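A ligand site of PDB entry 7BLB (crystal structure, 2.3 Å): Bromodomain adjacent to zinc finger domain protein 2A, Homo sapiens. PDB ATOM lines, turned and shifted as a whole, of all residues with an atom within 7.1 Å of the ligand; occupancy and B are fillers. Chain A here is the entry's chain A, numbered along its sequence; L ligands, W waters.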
ATOM      1  N   TRP A  23      18.878  12.361  13.148  1.00  0.00           N
ATOM      2  CA  TRP A  23      19.083  11.425  14.246  1.00  0.00           C
ATOM      3  C   TRP A  23      19.664  12.016  15.544  1.00  0.00           C
ATOM      4  O   TRP A  23      19.392  11.434  16.602  1.00  0.00           O
ATOM      5  CB  TRP A  23      19.950  10.253  13.759  1.00  0.00           C
ATOM      6  CG  TRP A  23      21.277  10.677  13.220  1.00  0.00           C
ATOM      7  CD1 TRP A  23      21.569  11.015  11.935  1.00  0.00           C
ATOM      8  CD2 TRP A  23      22.493  10.817  13.957  1.00  0.00           C
ATOM      9  NE1 TRP A  23      22.895  11.363  11.823  1.00  0.00           N
ATOM     10  CE2 TRP A  23      23.486  11.259  13.054  1.00  0.00           C
ATOM     11  CE3 TRP A  23      22.841  10.633  15.305  1.00  0.00           C
ATOM     12  CZ2 TRP A  23      24.809  11.496  13.453  1.00  0.00           C
ATOM     13  CZ3 TRP A  23      24.145  10.877  15.705  1.00  0.00           C
ATOM     14  CH2 TRP A  23      25.121  11.299  14.776  1.00  0.00           C
ATOM     15  N   PRO A  24      20.465  13.099  15.554  1.00  0.00           N
ATOM     16  CA  PRO A  24      20.877  13.643  16.861  1.00  0.00           C
ATOM     17  C   PRO A  24      19.805  14.432  17.561  1.00  0.00           C
ATOM     18  O   PRO A  24      19.980  14.750  18.753  1.00  0.00           O
ATOM     19  CB  PRO A  24      22.072  14.556  16.504  1.00  0.00           C
ATOM     20  CG  PRO A  24      22.497  14.130  15.094  1.00  0.00           C
ATOM     21  CD  PRO A  24      21.193  13.761  14.450  1.00  0.00           C
ATOM     22  N   PHE A  25      18.686  14.731  16.909  1.00  0.00           N
ATOM     23  CA  PHE A  25      17.756  15.745  17.421  1.00  0.00           C
ATOM     24  C   PHE A  25      16.352  15.225  17.692  1.00  0.00           C
ATOM     25  O   PHE A  25      15.474  16.023  18.032  1.00  0.00           O
ATOM     26  CB  PHE A  25      17.705  16.933  16.465  1.00  0.00           C
ATOM     27  CG  PHE A  25      19.048  17.335  15.946  1.00  0.00           C
ATOM     28  CD1 PHE A  25      19.988  17.914  16.801  1.00  0.00           C
ATOM     29  CD2 PHE A  25      19.392  17.124  14.621  1.00  0.00           C
ATOM     30  CE1 PHE A  25      21.244  18.290  16.321  1.00  0.00           C
ATOM     31  CE2 PHE A  25      20.657  17.497  14.131  1.00  0.00           C
ATOM     32  CZ  PHE A  25      21.584  18.069  14.977  1.00  0.00           C
ATOM     33  N   LEU A  26      16.114  13.916  17.565  1.00  0.00           N
ATOM     34  CA  LEU A  26      14.759  13.414  17.729  1.00  0.00           C
ATOM     35  C   LEU A  26      14.340  13.355  19.199  1.00  0.00           C
ATOM     36  O   LEU A  26      13.142  13.384  19.496  1.00  0.00           O
ATOM     37  CB  LEU A  26      14.630  12.030  17.084  1.00  0.00           C
ATOM     38  CG  LEU A  26      14.996  11.863  15.603  1.00  0.00           C
ATOM     39  CD1 LEU A  26      15.080  10.385  15.256  1.00  0.00           C
ATOM     40  CD2 LEU A  26      13.977  12.549  14.705  1.00  0.00           C
ATOM     41  N   GLU A  27      15.295  13.293  20.133  1.00  0.00           N
ATOM     42  CA  GLU A  27      15.018  13.160  21.555  1.00  0.00           C
ATOM     43  C   GLU A  27      15.999  14.006  22.378  1.00  0.00           C
ATOM     44  O   GLU A  27      17.129  14.213  21.951  1.00  0.00           O
ATOM     45  CB  GLU A  27      15.131  11.691  21.990  1.00  0.00           C
ATOM     46  CG  GLU A  27      14.365  10.747  21.073  1.00  0.00           C
ATOM     47  CD  GLU A  27      13.659   9.654  21.830  1.00  0.00           C
ATOM     48  OE1 GLU A  27      14.354   8.812  22.444  1.00  0.00           O
ATOM     49  OE2 GLU A  27      12.397   9.683  21.821  1.00  0.00           O
ATOM     50  N   PRO A  28      15.595  14.449  23.564  1.00  0.00           N
ATOM     51  CA  PRO A  28      16.495  15.265  24.387  1.00  0.00           C
ATOM     52  C   PRO A  28      17.821  14.584  24.632  1.00  0.00           C
ATOM     53  O   PRO A  28      17.892  13.365  24.824  1.00  0.00           O
ATOM     54  CB  PRO A  28      15.715  15.447  25.703  1.00  0.00           C
ATOM     55  CG  PRO A  28      14.295  15.228  25.332  1.00  0.00           C
ATOM     56  CD  PRO A  28      14.322  14.180  24.259  1.00  0.00           C
ATOM     57  N   VAL A  29      18.894  15.382  24.605  1.00  0.00           N
ATOM     58  CA  VAL A  29      20.199  14.852  24.974  1.00  0.00           C
ATOM     59  C   VAL A  29      20.136  14.362  26.409  1.00  0.00           C
ATOM     60  O   VAL A  29      19.472  14.970  27.266  1.00  0.00           O
ATOM     61  CB  VAL A  29      21.296  15.923  24.807  1.00  0.00           C
ATOM     62  CG1 VAL A  29      22.629  15.395  25.274  1.00  0.00           C
ATOM     63  CG2 VAL A  29      21.414  16.388  23.359  1.00  0.00           C
ATOM     64  N   ASN A  30      20.789  13.231  26.684  1.00  0.00           N
ATOM     65  CA  ASN A  30      20.786  12.684  28.027  1.00  0.00           C
ATOM     66  C   ASN A  30      22.039  13.146  28.750  1.00  0.00           C
ATOM     67  O   ASN A  30      23.134  12.628  28.483  1.00  0.00           O
ATOM     68  CB  ASN A  30      20.716  11.163  28.009  1.00  0.00           C
ATOM     69  CG  ASN A  30      20.342  10.583  29.367  1.00  0.00           C
ATOM     70  OD1 ASN A  30      20.563  11.218  30.414  1.00  0.00           O
ATOM     71  ND2 ASN A  30      19.760   9.389  29.365  1.00  0.00           N
ATOM     72  N   LEU A  33      24.646  10.763  29.793  1.00  0.00           N
ATOM     73  CA  LEU A  33      25.467  10.127  28.763  1.00  0.00           C
ATOM     74  C   LEU A  33      26.415  11.099  28.073  1.00  0.00           C
ATOM     75  O   LEU A  33      27.367  10.649  27.432  1.00  0.00           O
ATOM     76  CB  LEU A  33      24.569   9.457  27.709  1.00  0.00           C
ATOM     77  CG  LEU A  33      23.579   8.460  28.335  1.00  0.00           C
ATOM     78  CD1 LEU A  33      22.570   7.938  27.332  1.00  0.00           C
ATOM     79  CD2 LEU A  33      24.321   7.321  29.024  1.00  0.00           C
ATOM     80  N   VAL A  34      26.227  12.402  28.238  1.00  0.00           N
ATOM     81  CA  VAL A  34      26.991  13.398  27.502  1.00  0.00           C
ATOM     82  C   VAL A  34      27.671  14.311  28.510  1.00  0.00           C
ATOM     83  O   VAL A  34      27.059  15.271  29.017  1.00  0.00           O
ATOM     84  CB  VAL A  34      26.118  14.183  26.515  1.00  0.00           C
ATOM     85  CG1 VAL A  34      26.966  15.128  25.694  1.00  0.00           C
ATOM     86  CG2 VAL A  34      25.352  13.198  25.610  1.00  0.00           C
ATOM     87  N   SER A  35      28.944  14.031  28.775  1.00  0.00           N
ATOM     88  CA  SER A  35      29.677  14.754  29.800  1.00  0.00           C
ATOM     89  C   SER A  35      29.797  16.218  29.434  1.00  0.00           C
ATOM     90  O   SER A  35      30.102  16.565  28.288  1.00  0.00           O
ATOM     91  CB  SER A  35      31.068  14.132  29.975  1.00  0.00           C
ATOM     92  OG  SER A  35      31.976  15.095  30.486  1.00  0.00           O
ATOM     93  N   TYR A  37      27.376  18.417  29.231  1.00  0.00           N
ATOM     94  CA  TYR A  37      26.291  18.985  28.448  1.00  0.00           C
ATOM     95  C   TYR A  37      25.475  19.995  29.252  1.00  0.00           C
ATOM     96  O   TYR A  37      25.183  21.092  28.766  1.00  0.00           O
ATOM     97  CB  TYR A  37      25.375  17.895  27.886  1.00  0.00           C
ATOM     98  CG  TYR A  37      24.539  18.405  26.732  1.00  0.00           C
ATOM     99  CD1 TYR A  37      25.092  18.526  25.436  1.00  0.00           C
ATOM    100  CD2 TYR A  37      23.228  18.808  26.915  1.00  0.00           C
ATOM    101  CE1 TYR A  37      24.331  19.023  24.367  1.00  0.00           C
ATOM    102  CE2 TYR A  37      22.471  19.316  25.864  1.00  0.00           C
ATOM    103  CZ  TYR A  37      23.018  19.409  24.592  1.00  0.00           C
ATOM    104  OH  TYR A  37      22.261  19.909  23.562  1.00  0.00           O
ATOM    105  N   ILE A  41      25.224  23.774  27.818  1.00  0.00           N
ATOM    106  CA  ILE A  41      23.984  24.068  27.096  1.00  0.00           C
ATOM    107  C   ILE A  41      22.954  24.470  28.139  1.00  0.00           C
ATOM    108  O   ILE A  41      22.478  23.639  28.919  1.00  0.00           O
ATOM    109  CB  ILE A  41      23.528  22.870  26.257  1.00  0.00           C
ATOM    110  CG1 ILE A  41      24.467  22.667  25.069  1.00  0.00           C
ATOM    111  CG2 ILE A  41      22.085  23.051  25.752  1.00  0.00           C
ATOM    112  CD1 ILE A  41      24.572  23.879  24.168  1.00  0.00           C
ATOM    113  N   MET A  45      17.001  21.772  23.666  1.00  0.00           N
ATOM    114  CA  MET A  45      15.832  21.721  22.799  1.00  0.00           C
ATOM    115  C   MET A  45      16.010  20.607  21.787  1.00  0.00           C
ATOM    116  O   MET A  45      17.136  20.259  21.426  1.00  0.00           O
ATOM    117  CB  MET A  45      15.602  23.064  22.101  1.00  0.00           C
ATOM    118  CG  MET A  45      14.350  23.162  21.242  1.00  0.00           C
ATOM    119  SD  MET A  45      12.814  22.695  22.074  1.00  0.00           S
ATOM    120  CE  MET A  45      12.850  23.710  23.565  1.00  0.00           C
ATOM    121  N   VAL A  72      17.784  24.475  18.514  1.00  0.00           N
ATOM    122  CA  VAL A  72      18.379  23.144  18.334  1.00  0.00           C
ATOM    123  C   VAL A  72      19.757  23.254  17.690  1.00  0.00           C
ATOM    124  O   VAL A  72      20.740  22.664  18.152  1.00  0.00           O
ATOM    125  CB  VAL A  72      17.461  22.228  17.509  1.00  0.00           C
ATOM    126  CG1 VAL A  72      18.137  20.878  17.363  1.00  0.00           C
ATOM    127  CG2 VAL A  72      16.097  22.053  18.166  1.00  0.00           C
ATOM    128  N   ASN A  75      22.405  25.221  19.841  1.00  0.00           N
ATOM    129  CA  ASN A  75      22.949  24.297  20.837  1.00  0.00           C
ATOM    130  C   ASN A  75      23.854  23.267  20.197  1.00  0.00           C
ATOM    131  O   ASN A  75      24.868  22.867  20.785  1.00  0.00           O
ATOM    132  CB  ASN A  75      21.823  23.567  21.598  1.00  0.00           C
ATOM    133  CG  ASN A  75      20.954  24.490  22.433  1.00  0.00           C
ATOM    134  OD1 ASN A  75      21.375  25.565  22.830  1.00  0.00           O
ATOM    135  ND2 ASN A  75      19.710  24.069  22.672  1.00  0.00           N
ATOM    136  N   CYS A  76      23.515  22.815  18.978  1.00  0.00           N
ATOM    137  CA  CYS A  76      24.343  21.814  18.303  1.00  0.00           C
ATOM    138  C   CYS A  76      25.726  22.379  17.992  1.00  0.00           C
ATOM    139  O   CYS A  76      26.749  21.728  18.243  1.00  0.00           O
ATOM    140  CB  CYS A  76      23.662  21.345  17.016  1.00  0.00           C
ATOM    141  SG  CYS A  76      24.667  20.140  16.117  1.00  0.00           S
ATOM    142  N   GLN A  77      25.765  23.574  17.399  1.00  0.00           N
ATOM    143  CA  GLN A  77      27.037  24.230  17.072  1.00  0.00           C
ATOM    144  C   GLN A  77      27.788  24.657  18.335  1.00  0.00           C
ATOM    145  O   GLN A  77      29.022  24.636  18.356  1.00  0.00           O
ATOM    146  CB  GLN A  77      26.785  25.435  16.163  1.00  0.00           C
ATOM    147  CG  GLN A  77      26.263  25.080  14.774  1.00  0.00           C
ATOM    148  CD  GLN A  77      25.821  26.283  13.963  1.00  0.00           C
ATOM    149  OE1 GLN A  77      26.601  26.857  13.202  1.00  0.00           O
ATOM    150  NE2 GLN A  77      24.543  26.663  14.114  1.00  0.00           N
ATOM    151  N   PHE A  79      27.951  22.944  21.115  1.00  0.00           N
ATOM    152  CA  PHE A  79      28.546  21.802  21.788  1.00  0.00           C
ATOM    153  C   PHE A  79      29.412  20.917  20.901  1.00  0.00           C
ATOM    154  O   PHE A  79      30.361  20.309  21.407  1.00  0.00           O
ATOM    155  CB  PHE A  79      27.459  20.938  22.444  1.00  0.00           C
ATOM    156  CG  PHE A  79      27.997  20.012  23.511  1.00  0.00           C
ATOM    157  CD1 PHE A  79      27.991  20.391  24.845  1.00  0.00           C
ATOM    158  CD2 PHE A  79      28.505  18.783  23.171  1.00  0.00           C
ATOM    159  CE1 PHE A  79      28.492  19.549  25.799  1.00  0.00           C
ATOM    160  CE2 PHE A  79      29.006  17.933  24.145  1.00  0.00           C
ATOM    161  CZ  PHE A  79      28.996  18.309  25.440  1.00  0.00           C
ATOM    162  N   ASN A  80      29.106  20.792  19.608  1.00  0.00           N
ATOM    163  CA  ASN A  80      29.830  19.884  18.726  1.00  0.00           C
ATOM    164  C   ASN A  80      30.691  20.655  17.734  1.00  0.00           C
ATOM    165  O   ASN A  80      30.282  21.711  17.241  1.00  0.00           O
ATOM    166  CB  ASN A  80      28.857  18.978  17.955  1.00  0.00           C
ATOM    167  CG  ASN A  80      27.868  18.287  18.873  1.00  0.00           C
ATOM    168  OD1 ASN A  80      27.956  17.086  19.082  1.00  0.00           O
ATOM    169  ND2 ASN A  80      26.939  19.059  19.461  1.00  0.00           N
ATOM    170  N   VAL A  86      27.832  14.667  14.730  1.00  0.00           N
ATOM    171  CA  VAL A  86      26.630  15.411  15.103  1.00  0.00           C
ATOM    172  C   VAL A  86      26.644  16.795  14.450  1.00  0.00           C
ATOM    173  O   VAL A  86      25.668  17.224  13.837  1.00  0.00           O
ATOM    174  CB  VAL A  86      26.499  15.518  16.627  1.00  0.00           C
ATOM    175  CG1 VAL A  86      25.341  16.457  16.994  1.00  0.00           C
ATOM    176  CG2 VAL A  86      26.322  14.122  17.235  1.00  0.00           C
ATOM    177  N   GLY A  87      27.773  17.497  14.556  1.00  0.00           N
ATOM    178  CA  GLY A  87      27.880  18.796  13.930  1.00  0.00           C
ATOM    179  C   GLY A  87      27.562  18.751  12.443  1.00  0.00           C
ATOM    180  O   GLY A  87      26.773  19.565  11.939  1.00  0.00           O
HETATM  181  C1  LIG L   1      21.046   8.559  18.577  1.00  0.00           C
HETATM  182  C2  LIG L   1      21.368   7.560  17.666  1.00  0.00           C
HETATM  183  C3  LIG L   1      22.568   6.869  17.772  1.00  0.00           C
HETATM  184  C4  LIG L   1      23.444   7.169  18.801  1.00  0.00           C
HETATM  185  C5  LIG L   1      23.120   8.160  19.723  1.00  0.00           C
HETATM  186  C6  LIG L   1      18.706  11.290  22.186  1.00  0.00           C
HETATM  187  N1  LIG L   1      19.529  11.373  21.302  1.00  0.00           N
HETATM  188  C7  LIG L   1      20.489  12.365  21.705  1.00  0.00           C
HETATM  189  C8  LIG L   1      21.898  12.257  21.042  1.00  0.00           C
HETATM  190  C9  LIG L   1      21.979  11.193  20.066  1.00  0.00           C
HETATM  191  C10 LIG L   1      21.563   9.985  20.663  1.00  0.00           C
HETATM  192  C11 LIG L   1      20.044  10.044  21.018  1.00  0.00           C
HETATM  193  C12 LIG L   1      21.918   8.840  19.617  1.00  0.00           C
HETATM  194  N2  LIG L   1      22.254  13.534  20.345  1.00  0.00           N
HETATM  195  C13 LIG L   1      23.481  14.173  20.757  1.00  0.00           C
HETATM  196  C14 LIG L   1      24.549  13.357  21.387  1.00  0.00           C
HETATM  197  N3  LIG L   1      25.794  14.023  21.806  1.00  0.00           N
HETATM  198  N4  LIG L   1      25.960  15.458  21.609  1.00  0.00           N
HETATM  199  C15 LIG L   1      27.206  16.011  22.045  1.00  0.00           C
HETATM  200  C16 LIG L   1      24.920  16.290  21.006  1.00  0.00           C
HETATM  201  O1  LIG L   1      25.049  17.469  20.859  1.00  0.00           O
HETATM  202  C17 LIG L   1      23.660  15.616  20.569  1.00  0.00           C
HETATM  203 BR1  LIG L   1      22.243  16.646  19.746  1.00  0.00          BR
HETATM  204  O   HOH W   1      18.207  12.101  19.232  1.00  0.00           O
HETATM  205  O   HOH W   2      23.522  19.857  21.067  1.00  0.00           O
HETATM  206  O   HOH W   3      21.771  11.299  24.535  1.00  0.00           O
HETATM  207  O   HOH W   4      19.026  16.047  20.869  1.00  0.00           O
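The backbone carbonyl oxygen (O) of Pro 24 lies within hydrogen-bond range of a nitrogen (N2) of the ligand, at 3.0 Å.
The side-chain amide nitrogen of Asn 80 lies within hydrogen-bond range of an oxygen (O1) of the ligand (2.8 Å).
The side-chain amide nitrogen (ND2) of Asn 80 is in hydrogen-bond range of the backbone carbonyl oxygen (O) of Cys 76.
Trp 23 touches the ligand (O to C1, 3.9 Å).
Phe 25 touches the ligand (CD1 to BR1, 3.9 Å).
O of Glu 27 touches C6 of the ligand, 3.3 Å away.
O of Pro 28 touches C6 of the ligand (3.5 Å).
Val 29 touches the ligand.
Val 34 touches the ligand.
CE1 of Tyr 37 touches O1 of the ligand (3.9 Å).
Phe 79 touches the ligand.
Hydrophobic or aromatic side chains that line the ligand: Pro 24, Phe 25, Val 29, Val 34, Tyr 37 and Phe 79.
Within 4 Å of the ligand: Trp 23, Pro 24, Phe 25, Glu 27, Pro 28, Val 29, Val 34, Tyr 37, Phe 79 and Asn 80.
Water W2 lies within hydrogen-bond range of OH of Tyr 37 (2.8 Å), O1 of the ligand (2.8 Å) and O of Asn 75 (3.3 Å).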
